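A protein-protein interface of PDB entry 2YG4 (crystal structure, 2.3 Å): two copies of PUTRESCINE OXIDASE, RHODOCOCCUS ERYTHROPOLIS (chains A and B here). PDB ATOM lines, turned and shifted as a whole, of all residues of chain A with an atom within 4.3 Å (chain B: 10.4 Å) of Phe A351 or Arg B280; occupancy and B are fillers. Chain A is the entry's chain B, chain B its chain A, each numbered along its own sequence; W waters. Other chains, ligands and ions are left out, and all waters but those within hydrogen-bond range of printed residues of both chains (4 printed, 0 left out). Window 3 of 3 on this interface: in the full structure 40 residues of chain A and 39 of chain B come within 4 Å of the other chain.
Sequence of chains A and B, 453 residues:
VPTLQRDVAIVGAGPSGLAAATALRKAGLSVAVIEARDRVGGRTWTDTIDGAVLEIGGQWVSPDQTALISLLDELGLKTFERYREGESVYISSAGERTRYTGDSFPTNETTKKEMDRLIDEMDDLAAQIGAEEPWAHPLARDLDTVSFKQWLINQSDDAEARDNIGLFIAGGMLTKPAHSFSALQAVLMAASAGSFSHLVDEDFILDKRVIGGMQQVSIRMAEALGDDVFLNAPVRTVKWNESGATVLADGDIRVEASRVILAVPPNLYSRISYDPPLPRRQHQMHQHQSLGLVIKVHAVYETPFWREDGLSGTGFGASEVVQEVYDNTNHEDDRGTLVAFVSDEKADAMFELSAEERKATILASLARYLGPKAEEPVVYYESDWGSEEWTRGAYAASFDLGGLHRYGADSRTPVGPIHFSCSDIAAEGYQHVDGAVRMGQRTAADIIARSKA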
ATOM      1  N   ILE A 295     -12.894 -19.872  12.028  1.00  0.00           N
ATOM      2  CA  ILE A 295     -13.063 -18.619  12.777  1.00  0.00           C
ATOM      3  C   ILE A 295     -11.704 -17.930  12.738  1.00  0.00           C
ATOM      4  O   ILE A 295     -10.719 -18.526  13.144  1.00  0.00           O
ATOM      5  CB  ILE A 295     -13.485 -18.844  14.277  1.00  0.00           C
ATOM      6  CG1 ILE A 295     -14.656 -19.812  14.397  1.00  0.00           C
ATOM      7  CG2 ILE A 295     -13.819 -17.506  14.985  1.00  0.00           C
ATOM      8  CD1 ILE A 295     -15.146 -20.065  15.821  1.00  0.00           C
ATOM      9  N   ALA A 347     -14.561 -25.240  14.734  1.00  0.00           N
ATOM     10  CA  ALA A 347     -15.342 -24.001  14.612  1.00  0.00           C
ATOM     11  C   ALA A 347     -16.805 -24.201  14.971  1.00  0.00           C
ATOM     12  O   ALA A 347     -17.374 -23.411  15.724  1.00  0.00           O
ATOM     13  CB  ALA A 347     -15.206 -23.382  13.150  1.00  0.00           C
ATOM     14  N   ASP A 348     -17.428 -25.270  14.464  1.00  0.00           N
ATOM     15  CA  ASP A 348     -18.859 -25.600  14.771  1.00  0.00           C
ATOM     16  C   ASP A 348     -19.035 -25.740  16.303  1.00  0.00           C
ATOM     17  O   ASP A 348     -20.019 -25.262  16.910  1.00  0.00           O
ATOM     18  CB  ASP A 348     -19.270 -26.974  14.210  1.00  0.00           C
ATOM     19  CG  ASP A 348     -19.169 -27.131  12.654  1.00  0.00           C
ATOM     20  OD1 ASP A 348     -18.624 -26.281  11.887  1.00  0.00           O
ATOM     21  OD2 ASP A 348     -19.639 -28.212  12.197  1.00  0.00           O
ATOM     22  N   ALA A 349     -18.068 -26.406  16.906  1.00  0.00           N
ATOM     23  CA  ALA A 349     -18.085 -26.706  18.324  1.00  0.00           C
ATOM     24  C   ALA A 349     -18.014 -25.382  19.101  1.00  0.00           C
ATOM     25  O   ALA A 349     -18.812 -25.183  19.977  1.00  0.00           O
ATOM     26  CB  ALA A 349     -16.873 -27.692  18.726  1.00  0.00           C
ATOM     27  N   MET A 350     -17.094 -24.474  18.740  1.00  0.00           N
ATOM     28  CA  MET A 350     -17.025 -23.169  19.384  1.00  0.00           C
ATOM     29  C   MET A 350     -18.288 -22.380  19.191  1.00  0.00           C
ATOM     30  O   MET A 350     -18.720 -21.653  20.121  1.00  0.00           O
ATOM     31  CB  MET A 350     -15.849 -22.367  18.846  1.00  0.00           C
ATOM     32  CG  MET A 350     -14.401 -22.864  19.327  1.00  0.00           C
ATOM     33  SD  MET A 350     -14.357 -23.040  21.158  1.00  0.00           S
ATOM     34  CE  MET A 350     -14.700 -24.842  21.423  1.00  0.00           C
ATOM     35  N   PHE A 351     -18.911 -22.475  18.002  1.00  0.00           N
ATOM     36  CA  PHE A 351     -20.120 -21.671  17.770  1.00  0.00           C
ATOM     37  C   PHE A 351     -21.328 -22.190  18.537  1.00  0.00           C
ATOM     38  O   PHE A 351     -22.294 -21.483  18.724  1.00  0.00           O
ATOM     39  CB  PHE A 351     -20.458 -21.593  16.274  1.00  0.00           C
ATOM     40  CG  PHE A 351     -19.616 -20.577  15.511  1.00  0.00           C
ATOM     41  CD1 PHE A 351     -19.538 -19.262  15.951  1.00  0.00           C
ATOM     42  CD2 PHE A 351     -18.933 -20.947  14.346  1.00  0.00           C
ATOM     43  CE1 PHE A 351     -18.801 -18.306  15.272  1.00  0.00           C
ATOM     44  CE2 PHE A 351     -18.185 -20.009  13.614  1.00  0.00           C
ATOM     45  CZ  PHE A 351     -18.104 -18.660  14.050  1.00  0.00           C
ATOM     46  N   GLU A 352     -21.281 -23.428  18.971  1.00  0.00           N
ATOM     47  CA  GLU A 352     -22.338 -23.925  19.804  1.00  0.00           C
ATOM     48  C   GLU A 352     -22.203 -23.446  21.250  1.00  0.00           C
ATOM     49  O   GLU A 352     -23.142 -23.597  21.985  1.00  0.00           O
ATOM     50  CB  GLU A 352     -22.382 -25.458  19.717  1.00  0.00           C
ATOM     51  CG  GLU A 352     -22.995 -25.886  18.331  1.00  0.00           C
ATOM     52  CD  GLU A 352     -22.898 -27.336  18.078  1.00  0.00           C
ATOM     53  OE1 GLU A 352     -22.983 -28.078  19.103  1.00  0.00           O
ATOM     54  OE2 GLU A 352     -22.733 -27.754  16.881  1.00  0.00           O
ATOM     55  N   LEU A 353     -21.052 -22.871  21.659  1.00  0.00           N
ATOM     56  CA  LEU A 353     -20.925 -22.359  23.027  1.00  0.00           C
ATOM     57  C   LEU A 353     -21.478 -20.972  22.983  1.00  0.00           C
ATOM     58  O   LEU A 353     -21.548 -20.345  21.890  1.00  0.00           O
ATOM     59  CB  LEU A 353     -19.458 -22.264  23.455  1.00  0.00           C
ATOM     60  CG  LEU A 353     -18.714 -23.593  23.572  1.00  0.00           C
ATOM     61  CD1 LEU A 353     -17.268 -23.364  23.904  1.00  0.00           C
ATOM     62  CD2 LEU A 353     -19.421 -24.467  24.661  1.00  0.00           C
ATOM     63  N   ARG A 358     -17.139 -19.281  24.515  1.00  0.00           N
ATOM     64  CA  ARG A 358     -16.334 -19.418  23.344  1.00  0.00           C
ATOM     65  C   ARG A 358     -15.039 -18.536  23.409  1.00  0.00           C
ATOM     66  O   ARG A 358     -13.912 -19.008  23.123  1.00  0.00           O
ATOM     67  CB  ARG A 358     -17.181 -19.063  22.080  1.00  0.00           C
ATOM     68  CG  ARG A 358     -16.326 -18.888  20.809  1.00  0.00           C
ATOM     69  CD  ARG A 358     -17.185 -18.893  19.506  1.00  0.00           C
ATOM     70  NE  ARG A 358     -18.040 -17.693  19.397  1.00  0.00           N
ATOM     71  CZ  ARG A 358     -19.337 -17.688  19.708  1.00  0.00           C
ATOM     72  NH1 ARG A 358     -19.987 -18.789  20.134  1.00  0.00           N
ATOM     73  NH2 ARG A 358     -19.992 -16.582  19.571  1.00  0.00           N
ATOM     74  N   ASP A 384     -16.862 -13.548  11.282  1.00  0.00           N
ATOM     75  CA  ASP A 384     -17.921 -14.530  11.149  1.00  0.00           C
ATOM     76  C   ASP A 384     -18.439 -14.586   9.705  1.00  0.00           C
ATOM     77  O   ASP A 384     -19.516 -14.152   9.422  1.00  0.00           O
ATOM     78  CB  ASP A 384     -19.039 -14.265  12.206  1.00  0.00           C
ATOM     79  CG  ASP A 384     -20.229 -15.249  12.083  1.00  0.00           C
ATOM     80  OD1 ASP A 384     -20.017 -16.409  11.562  1.00  0.00           O
ATOM     81  OD2 ASP A 384     -21.377 -14.844  12.467  1.00  0.00           O
ATOM     82  N   GLY A 386     -19.456 -17.210   8.001  1.00  0.00           N
ATOM     83  CA  GLY A 386     -20.494 -18.173   7.806  1.00  0.00           C
ATOM     84  C   GLY A 386     -21.888 -17.549   7.890  1.00  0.00           C
ATOM     85  O   GLY A 386     -22.794 -18.000   7.211  1.00  0.00           O
ATOM     86  N   SER A 387     -22.063 -16.518   8.714  1.00  0.00           N
ATOM     87  CA  SER A 387     -23.346 -15.836   8.832  1.00  0.00           C
ATOM     88  C   SER A 387     -23.677 -14.924   7.674  1.00  0.00           C
ATOM     89  O   SER A 387     -24.842 -14.539   7.500  1.00  0.00           O
ATOM     90  CB  SER A 387     -23.410 -14.979  10.126  1.00  0.00           C
ATOM     91  OG  SER A 387     -23.188 -15.832  11.234  1.00  0.00           O
ATOM     92  N   TRP B 240     -39.200 -12.867   7.598  1.00  0.00           N
ATOM     93  CA  TRP B 240     -39.738 -13.563   8.751  1.00  0.00           C
ATOM     94  C   TRP B 240     -39.254 -12.914  10.024  1.00  0.00           C
ATOM     95  O   TRP B 240     -38.245 -12.176  10.015  1.00  0.00           O
ATOM     96  CB  TRP B 240     -39.327 -15.054   8.746  1.00  0.00           C
ATOM     97  CG  TRP B 240     -37.764 -15.271   8.774  1.00  0.00           C
ATOM     98  CD1 TRP B 240     -36.898 -15.174   7.704  1.00  0.00           C
ATOM     99  CD2 TRP B 240     -36.943 -15.611   9.915  1.00  0.00           C
ATOM    100  NE1 TRP B 240     -35.635 -15.436   8.116  1.00  0.00           N
ATOM    101  CE2 TRP B 240     -35.629 -15.691   9.464  1.00  0.00           C
ATOM    102  CE3 TRP B 240     -37.212 -15.853  11.271  1.00  0.00           C
ATOM    103  CZ2 TRP B 240     -34.577 -15.985  10.297  1.00  0.00           C
ATOM    104  CZ3 TRP B 240     -36.136 -16.145  12.145  1.00  0.00           C
ATOM    105  CH2 TRP B 240     -34.836 -16.217  11.644  1.00  0.00           C
ATOM    106  N   PRO B 276     -34.643 -11.748   7.636  1.00  0.00           N
ATOM    107  CA  PRO B 276     -33.166 -11.741   7.648  1.00  0.00           C
ATOM    108  C   PRO B 276     -32.599 -13.127   7.181  1.00  0.00           C
ATOM    109  O   PRO B 276     -33.368 -14.115   7.105  1.00  0.00           O
ATOM    110  CB  PRO B 276     -32.851 -11.481   9.125  1.00  0.00           C
ATOM    111  CG  PRO B 276     -33.960 -12.182   9.838  1.00  0.00           C
ATOM    112  CD  PRO B 276     -35.192 -11.956   8.980  1.00  0.00           C
ATOM    113  N   PRO B 277     -31.290 -13.199   6.848  1.00  0.00           N
ATOM    114  CA  PRO B 277     -30.737 -14.509   6.372  1.00  0.00           C
ATOM    115  C   PRO B 277     -30.897 -15.679   7.377  1.00  0.00           C
ATOM    116  O   PRO B 277     -31.017 -15.444   8.603  1.00  0.00           O
ATOM    117  CB  PRO B 277     -29.248 -14.239   6.154  1.00  0.00           C
ATOM    118  CG  PRO B 277     -29.055 -12.776   6.195  1.00  0.00           C
ATOM    119  CD  PRO B 277     -30.301 -12.092   6.769  1.00  0.00           C
ATOM    120  N   LEU B 278     -30.869 -16.926   6.891  1.00  0.00           N
ATOM    121  CA  LEU B 278     -30.835 -18.058   7.798  1.00  0.00           C
ATOM    122  C   LEU B 278     -29.527 -17.984   8.601  1.00  0.00           C
ATOM    123  O   LEU B 278     -28.531 -17.386   8.126  1.00  0.00           O
ATOM    124  CB  LEU B 278     -30.957 -19.371   7.012  1.00  0.00           C
ATOM    125  CG  LEU B 278     -32.212 -19.568   6.121  1.00  0.00           C
ATOM    126  CD1 LEU B 278     -32.235 -20.913   5.464  1.00  0.00           C
ATOM    127  CD2 LEU B 278     -33.503 -19.357   6.906  1.00  0.00           C
ATOM    128  N   PRO B 279     -29.493 -18.608   9.788  1.00  0.00           N
ATOM    129  CA  PRO B 279     -28.252 -18.588  10.557  1.00  0.00           C
ATOM    130  C   PRO B 279     -27.144 -19.393   9.859  1.00  0.00           C
ATOM    131  O   PRO B 279     -27.388 -20.240   8.955  1.00  0.00           O
ATOM    132  CB  PRO B 279     -28.612 -19.341  11.859  1.00  0.00           C
ATOM    133  CG  PRO B 279     -30.169 -19.268  11.921  1.00  0.00           C
ATOM    134  CD  PRO B 279     -30.569 -19.361  10.478  1.00  0.00           C
ATOM    135  N   ARG B 280     -25.950 -19.143  10.339  1.00  0.00           N
ATOM    136  CA  ARG B 280     -24.744 -19.762   9.869  1.00  0.00           C
ATOM    137  C   ARG B 280     -24.905 -21.300   9.700  1.00  0.00           C
ATOM    138  O   ARG B 280     -24.425 -21.853   8.707  1.00  0.00           O
ATOM    139  CB  ARG B 280     -23.562 -19.375  10.838  1.00  0.00           C
ATOM    140  CG  ARG B 280     -22.405 -20.344  10.945  1.00  0.00           C
ATOM    141  CD  ARG B 280     -21.209 -19.952  11.880  1.00  0.00           C
ATOM    142  NE  ARG B 280     -21.396 -18.721  12.598  1.00  0.00           N
ATOM    143  CZ  ARG B 280     -22.065 -18.579  13.731  1.00  0.00           C
ATOM    144  NH1 ARG B 280     -22.623 -19.608  14.370  1.00  0.00           N
ATOM    145  NH2 ARG B 280     -22.168 -17.363  14.210  1.00  0.00           N
ATOM    146  N   ARG B 281     -25.543 -21.973  10.661  1.00  0.00           N
ATOM    147  CA  ARG B 281     -25.547 -23.428  10.670  1.00  0.00           C
ATOM    148  C   ARG B 281     -26.315 -23.940   9.456  1.00  0.00           C
ATOM    149  O   ARG B 281     -25.891 -24.885   8.831  1.00  0.00           O
ATOM    150  CB  ARG B 281     -26.170 -24.045  11.941  1.00  0.00           C
ATOM    151  CG  ARG B 281     -26.245 -25.578  11.840  1.00  0.00           C
ATOM    152  CD  ARG B 281     -24.779 -26.046  11.636  1.00  0.00           C
ATOM    153  NE  ARG B 281     -24.662 -26.863  12.753  1.00  0.00           N
ATOM    154  CZ  ARG B 281     -23.921 -26.718  13.824  1.00  0.00           C
ATOM    155  NH1 ARG B 281     -22.955 -25.820  13.971  1.00  0.00           N
ATOM    156  NH2 ARG B 281     -24.166 -27.618  14.739  1.00  0.00           N
ATOM    157  N   GLN B 282     -27.440 -23.301   9.144  1.00  0.00           N
ATOM    158  CA  GLN B 282     -28.147 -23.585   7.901  1.00  0.00           C
ATOM    159  C   GLN B 282     -27.314 -23.175   6.641  1.00  0.00           C
ATOM    160  O   GLN B 282     -27.232 -23.912   5.664  1.00  0.00           O
ATOM    161  CB  GLN B 282     -29.528 -22.878   7.931  1.00  0.00           C
ATOM    162  CG  GLN B 282     -30.587 -23.624   8.754  1.00  0.00           C
ATOM    163  CD  GLN B 282     -30.269 -23.611  10.243  1.00  0.00           C
ATOM    164  OE1 GLN B 282     -29.626 -22.680  10.726  1.00  0.00           O
ATOM    165  NE2 GLN B 282     -30.745 -24.622  10.985  1.00  0.00           N
ATOM    166  N   HIS B 283     -26.667 -22.015   6.691  1.00  0.00           N
ATOM    167  CA  HIS B 283     -25.863 -21.577   5.541  1.00  0.00           C
ATOM    168  C   HIS B 283     -24.863 -22.671   5.154  1.00  0.00           C
ATOM    169  O   HIS B 283     -24.686 -22.997   3.952  1.00  0.00           O
ATOM    170  CB  HIS B 283     -25.057 -20.329   5.894  1.00  0.00           C
ATOM    171  CG  HIS B 283     -25.792 -19.025   5.724  1.00  0.00           C
ATOM    172  ND1 HIS B 283     -27.008 -18.915   5.056  1.00  0.00           N
ATOM    173  CD2 HIS B 283     -25.459 -17.765   6.120  1.00  0.00           C
ATOM    174  CE1 HIS B 283     -27.376 -17.640   5.016  1.00  0.00           C
ATOM    175  NE2 HIS B 283     -26.463 -16.926   5.668  1.00  0.00           N
ATOM    176  N   GLN B 284     -24.220 -23.246   6.182  1.00  0.00           N
ATOM    177  CA  GLN B 284     -23.199 -24.276   6.003  1.00  0.00           C
ATOM    178  C   GLN B 284     -23.803 -25.624   5.623  1.00  0.00           C
ATOM    179  O   GLN B 284     -23.401 -26.210   4.642  1.00  0.00           O
ATOM    180  CB  GLN B 284     -22.323 -24.407   7.260  1.00  0.00           C
ATOM    181  CG  GLN B 284     -21.345 -23.271   7.412  1.00  0.00           C
ATOM    182  CD  GLN B 284     -19.985 -23.628   6.814  1.00  0.00           C
ATOM    183  OE1 GLN B 284     -19.485 -22.942   5.890  1.00  0.00           O
ATOM    184  NE2 GLN B 284     -19.405 -24.752   7.266  1.00  0.00           N
ATOM    185  N   MET B 285     -24.744 -26.108   6.407  1.00  0.00           N
ATOM    186  CA  MET B 285     -25.325 -27.424   6.186  1.00  0.00           C
ATOM    187  C   MET B 285     -25.891 -27.556   4.798  1.00  0.00           C
ATOM    188  O   MET B 285     -25.734 -28.588   4.185  1.00  0.00           O
ATOM    189  CB  MET B 285     -26.439 -27.659   7.189  1.00  0.00           C
ATOM    190  CG  MET B 285     -27.332 -28.917   6.916  1.00  0.00           C
ATOM    191  SD  MET B 285     -28.465 -29.197   8.317  1.00  0.00           S
ATOM    192  CE  MET B 285     -29.190 -27.566   8.658  1.00  0.00           C
ATOM    193  N   HIS B 286     -26.572 -26.511   4.299  1.00  0.00           N
ATOM    194  CA  HIS B 286     -27.272 -26.615   3.035  1.00  0.00           C
ATOM    195  C   HIS B 286     -26.311 -26.766   1.888  1.00  0.00           C
ATOM    196  O   HIS B 286     -26.669 -27.385   0.880  1.00  0.00           O
ATOM    197  CB  HIS B 286     -28.188 -25.418   2.797  1.00  0.00           C
ATOM    198  CG  HIS B 286     -29.315 -25.332   3.783  1.00  0.00           C
ATOM    199  ND1 HIS B 286     -30.114 -24.212   3.912  1.00  0.00           N
ATOM    200  CD2 HIS B 286     -29.772 -26.231   4.694  1.00  0.00           C
ATOM    201  CE1 HIS B 286     -31.007 -24.422   4.863  1.00  0.00           C
ATOM    202  NE2 HIS B 286     -30.830 -25.645   5.344  1.00  0.00           N
ATOM    203  N   GLN B 287     -25.080 -26.260   2.038  1.00  0.00           N
ATOM    204  CA  GLN B 287     -24.027 -26.435   1.008  1.00  0.00           C
ATOM    205  C   GLN B 287     -23.541 -27.859   0.940  1.00  0.00           C
ATOM    206  O   GLN B 287     -22.926 -28.248  -0.052  1.00  0.00           O
ATOM    207  CB  GLN B 287     -22.802 -25.518   1.295  1.00  0.00           C
ATOM    208  CG  GLN B 287     -23.093 -24.061   1.197  1.00  0.00           C
ATOM    209  CD  GLN B 287     -21.889 -23.223   1.533  1.00  0.00           C
ATOM    210  OE1 GLN B 287     -20.850 -23.292   0.846  1.00  0.00           O
ATOM    211  NE2 GLN B 287     -22.018 -22.387   2.577  1.00  0.00           N
ATOM    212  N   HIS B 288     -23.763 -28.648   1.992  1.00  0.00           N
ATOM    213  CA  HIS B 288     -23.262 -30.022   1.981  1.00  0.00           C
ATOM    214  C   HIS B 288     -24.263 -31.092   1.551  1.00  0.00           C
ATOM    215  O   HIS B 288     -24.017 -32.292   1.746  1.00  0.00           O
ATOM    216  CB  HIS B 288     -22.684 -30.338   3.347  1.00  0.00           C
ATOM    217  CG  HIS B 288     -21.432 -29.555   3.664  1.00  0.00           C
ATOM    218  ND1 HIS B 288     -20.179 -29.972   3.302  1.00  0.00           N
ATOM    219  CD2 HIS B 288     -21.255 -28.370   4.277  1.00  0.00           C
ATOM    220  CE1 HIS B 288     -19.274 -29.116   3.739  1.00  0.00           C
ATOM    221  NE2 HIS B 288     -19.909 -28.132   4.342  1.00  0.00           N
ATOM    222  N   ARG B 406     -21.889 -34.626  10.956  1.00  0.00           N
ATOM    223  CA  ARG B 406     -21.637 -33.255  11.348  1.00  0.00           C
ATOM    224  C   ARG B 406     -22.941 -32.410  11.453  1.00  0.00           C
ATOM    225  O   ARG B 406     -23.053 -31.516  12.292  1.00  0.00           O
ATOM    226  CB  ARG B 406     -20.687 -32.636  10.323  1.00  0.00           C
ATOM    227  CG  ARG B 406     -20.140 -31.317  10.729  1.00  0.00           C
ATOM    228  CD  ARG B 406     -19.076 -30.827   9.686  1.00  0.00           C
ATOM    229  NE  ARG B 406     -18.684 -29.438   9.985  1.00  0.00           N
ATOM    230  CZ  ARG B 406     -17.777 -28.767   9.285  1.00  0.00           C
ATOM    231  NH1 ARG B 406     -17.202 -29.356   8.247  1.00  0.00           N
ATOM    232  NH2 ARG B 406     -17.444 -27.526   9.605  1.00  0.00           N
ATOM    233  N   TYR B 407     -23.877 -32.700  10.562  1.00  0.00           N
ATOM    234  CA  TYR B 407     -25.109 -31.856  10.375  1.00  0.00           C
ATOM    235  C   TYR B 407     -26.449 -32.529  10.588  1.00  0.00           C
ATOM    236  O   TYR B 407     -27.466 -31.832  10.647  1.00  0.00           O
ATOM    237  CB  TYR B 407     -25.150 -31.230   8.970  1.00  0.00           C
ATOM    238  CG  TYR B 407     -23.956 -30.344   8.678  1.00  0.00           C
ATOM    239  CD1 TYR B 407     -23.727 -29.176   9.417  1.00  0.00           C
ATOM    240  CD2 TYR B 407     -23.060 -30.711   7.668  1.00  0.00           C
ATOM    241  CE1 TYR B 407     -22.630 -28.349   9.163  1.00  0.00           C
ATOM    242  CE2 TYR B 407     -21.934 -29.953   7.401  1.00  0.00           C
ATOM    243  CZ  TYR B 407     -21.749 -28.742   8.109  1.00  0.00           C
ATOM    244  OH  TYR B 407     -20.633 -27.998   7.789  1.00  0.00           O
ATOM    245  N   ASP B 410     -29.148 -31.321  12.868  1.00  0.00           N
ATOM    246  CA  ASP B 410     -29.783 -30.063  12.502  1.00  0.00           C
ATOM    247  C   ASP B 410     -30.718 -30.085  11.291  1.00  0.00           C
ATOM    248  O   ASP B 410     -31.396 -29.081  11.022  1.00  0.00           O
ATOM    249  CB  ASP B 410     -28.730 -29.008  12.273  1.00  0.00           C
ATOM    250  CG  ASP B 410     -27.781 -28.870  13.479  1.00  0.00           C
ATOM    251  OD1 ASP B 410     -28.253 -28.617  14.603  1.00  0.00           O
ATOM    252  OD2 ASP B 410     -26.546 -29.044  13.308  1.00  0.00           O
ATOM    253  N   VAL B 415     -36.244 -23.011  11.858  1.00  0.00           N
ATOM    254  CA  VAL B 415     -35.604 -21.740  12.127  1.00  0.00           C
ATOM    255  C   VAL B 415     -36.719 -20.756  12.397  1.00  0.00           C
ATOM    256  O   VAL B 415     -37.465 -20.346  11.455  1.00  0.00           O
ATOM    257  CB  VAL B 415     -34.793 -21.304  10.917  1.00  0.00           C
ATOM    258  CG1 VAL B 415     -34.459 -19.770  10.987  1.00  0.00           C
ATOM    259  CG2 VAL B 415     -33.503 -22.171  10.817  1.00  0.00           C
HETATM  260  O   HOH W   1     -21.376 -29.827  13.497  1.00  0.00           O
HETATM  261  O   HOH W   2     -25.602 -16.811  12.161  1.00  0.00           O
HETATM  262  O   HOH W   3     -20.100 -25.813   9.317  1.00  0.00           O
HETATM  263  O   HOH W   4     -26.943 -15.525   9.074  1.00  0.00           O
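Hydrophobic or aromatic side chains of chain A that line the printed part of chain B: Phe A351. Of the 18 printed residues of chain B, 4 touch a printed residue of chain A. Printed residues of chain B that touch a printed residue of chain A: Arg B280, Arg B281, His B283 and Arg B406. Hydrophobic or aromatic side chains of chain B that line the printed part of chain A: His B283. Along chain B the printed residues that touch a printed residue of chain A span positions 280 to 406. Among the printed residues, Asp or Glu carboxylates within 4 Å of a Lys or Arg side-chain nitrogen of the other chain: Asp A348 with Arg B406, Glu A352 with Arg B281 and Asp A384 with Arg B280.
The backbone carbonyl oxygen (O) of Leu B278 lies within hydrogen-bond range of a ring nitrogen (NE2) of His B283 (3.2 Å). The guanidinium group of Arg B281 is in salt-bridge range of the side-chain carboxylate of Asp B410 (2.9 Å). NE2 of Gln B287 is in hydrogen-bond range of O of His B283 (3.1 Å). The guanidinium group (NE) of Arg B406 is in hydrogen-bond range of the side-chain hydroxyl (OH) of Tyr B407 (3.3 Å). The side-chain carboxylate (OD2) of Asp A384 sits at hydrogen-bond distance from the side-chain hydroxyl (OG) of Ser A387.
Ala A347 touches none of the printed residues of chain B. Printed residues of chain B within 4 Å of Asp A348: Arg B281 (3.9 Å) and Arg B406 (2.7 Å). No residue of chain B comes within 4 Å of Ala A349. No residue of chain B comes within 4 Å of Met A350. Phe A351 touches one residue of chain B. Of chain B, only Arg B281 comes within 4 Å of Glu A352. Arg B280 touches just these residues of chain A: Phe A351, Asp A384, Gly A386 and Ser A387. Printed residues of chain A within 4 Å of His B283: Gly A386 (2.9 Å) and Ser A387 (3.4 Å). Met B285 touches none of the printed residues of chain A. His B286 touches none of the printed residues of chain A. Of the printed residues of chain A, Arg B406 touches Asp A348. The nearest residue of chain B that does not touch Phe A351 is Arg B281 (5.4 Å). The nearest printed residue of chain A that does not touch Arg B280 is Arg A358 (5.8 Å). The nearest printed residue of chain A that does not touch Arg B281 is Phe A351 (5.4 Å).
Among the printed residues, pairs that only touch across the chains: Gly A386 with His B283, Phe A351 with Arg B280, Gly A386 with Arg B280 and Asp A348 with Arg B281.
The guanidinium group (NE) of Arg B280 is in salt-bridge range of the side-chain carboxylate (OD1) of Asp A384 (2.9 Å). The side-chain hydroxyl (OG) of Ser A387 is in hydrogen-bond range of the guanidinium group (NH2) of Arg B280 (3.5 Å). The guanidinium group of Arg B281 is in salt-bridge range of the side-chain carboxylate of Glu A352, 2.6 Å away. A ring nitrogen (NE2) of His B283 lies within hydrogen-bond range of the backbone carbonyl oxygen (O) of Ser A387 (3.4 Å). OD2 of Asp A348 is in salt-bridge range of NE of Arg B406 (2.7 Å).
Water W3 lies within hydrogen-bond range of NE2 of Gln B284 (2.4 Å), OH of Tyr B407 (2.7 Å), OD1 of Asp A348 (3.0 Å) and NH2 of Arg B406 (3.2 Å). Water W4 lies within hydrogen-bond range of O of Leu B278 and O of Ser A387. Water W1 lies within hydrogen-bond range of the backbone carbonyl oxygen (O) of Arg B406 and the side-chain carboxylate (OD2) of Asp A348. Water W2 lies within hydrogen-bond range of the side-chain hydroxyl (OG) of Ser A387 (2.8 Å) and the backbone NH (N) of Arg B280 (3.0 Å).
No position is printed for both chains. Of the 9 pairs that touch across the chains among the printed residues, none has its exchanged pair printed and touching as well.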
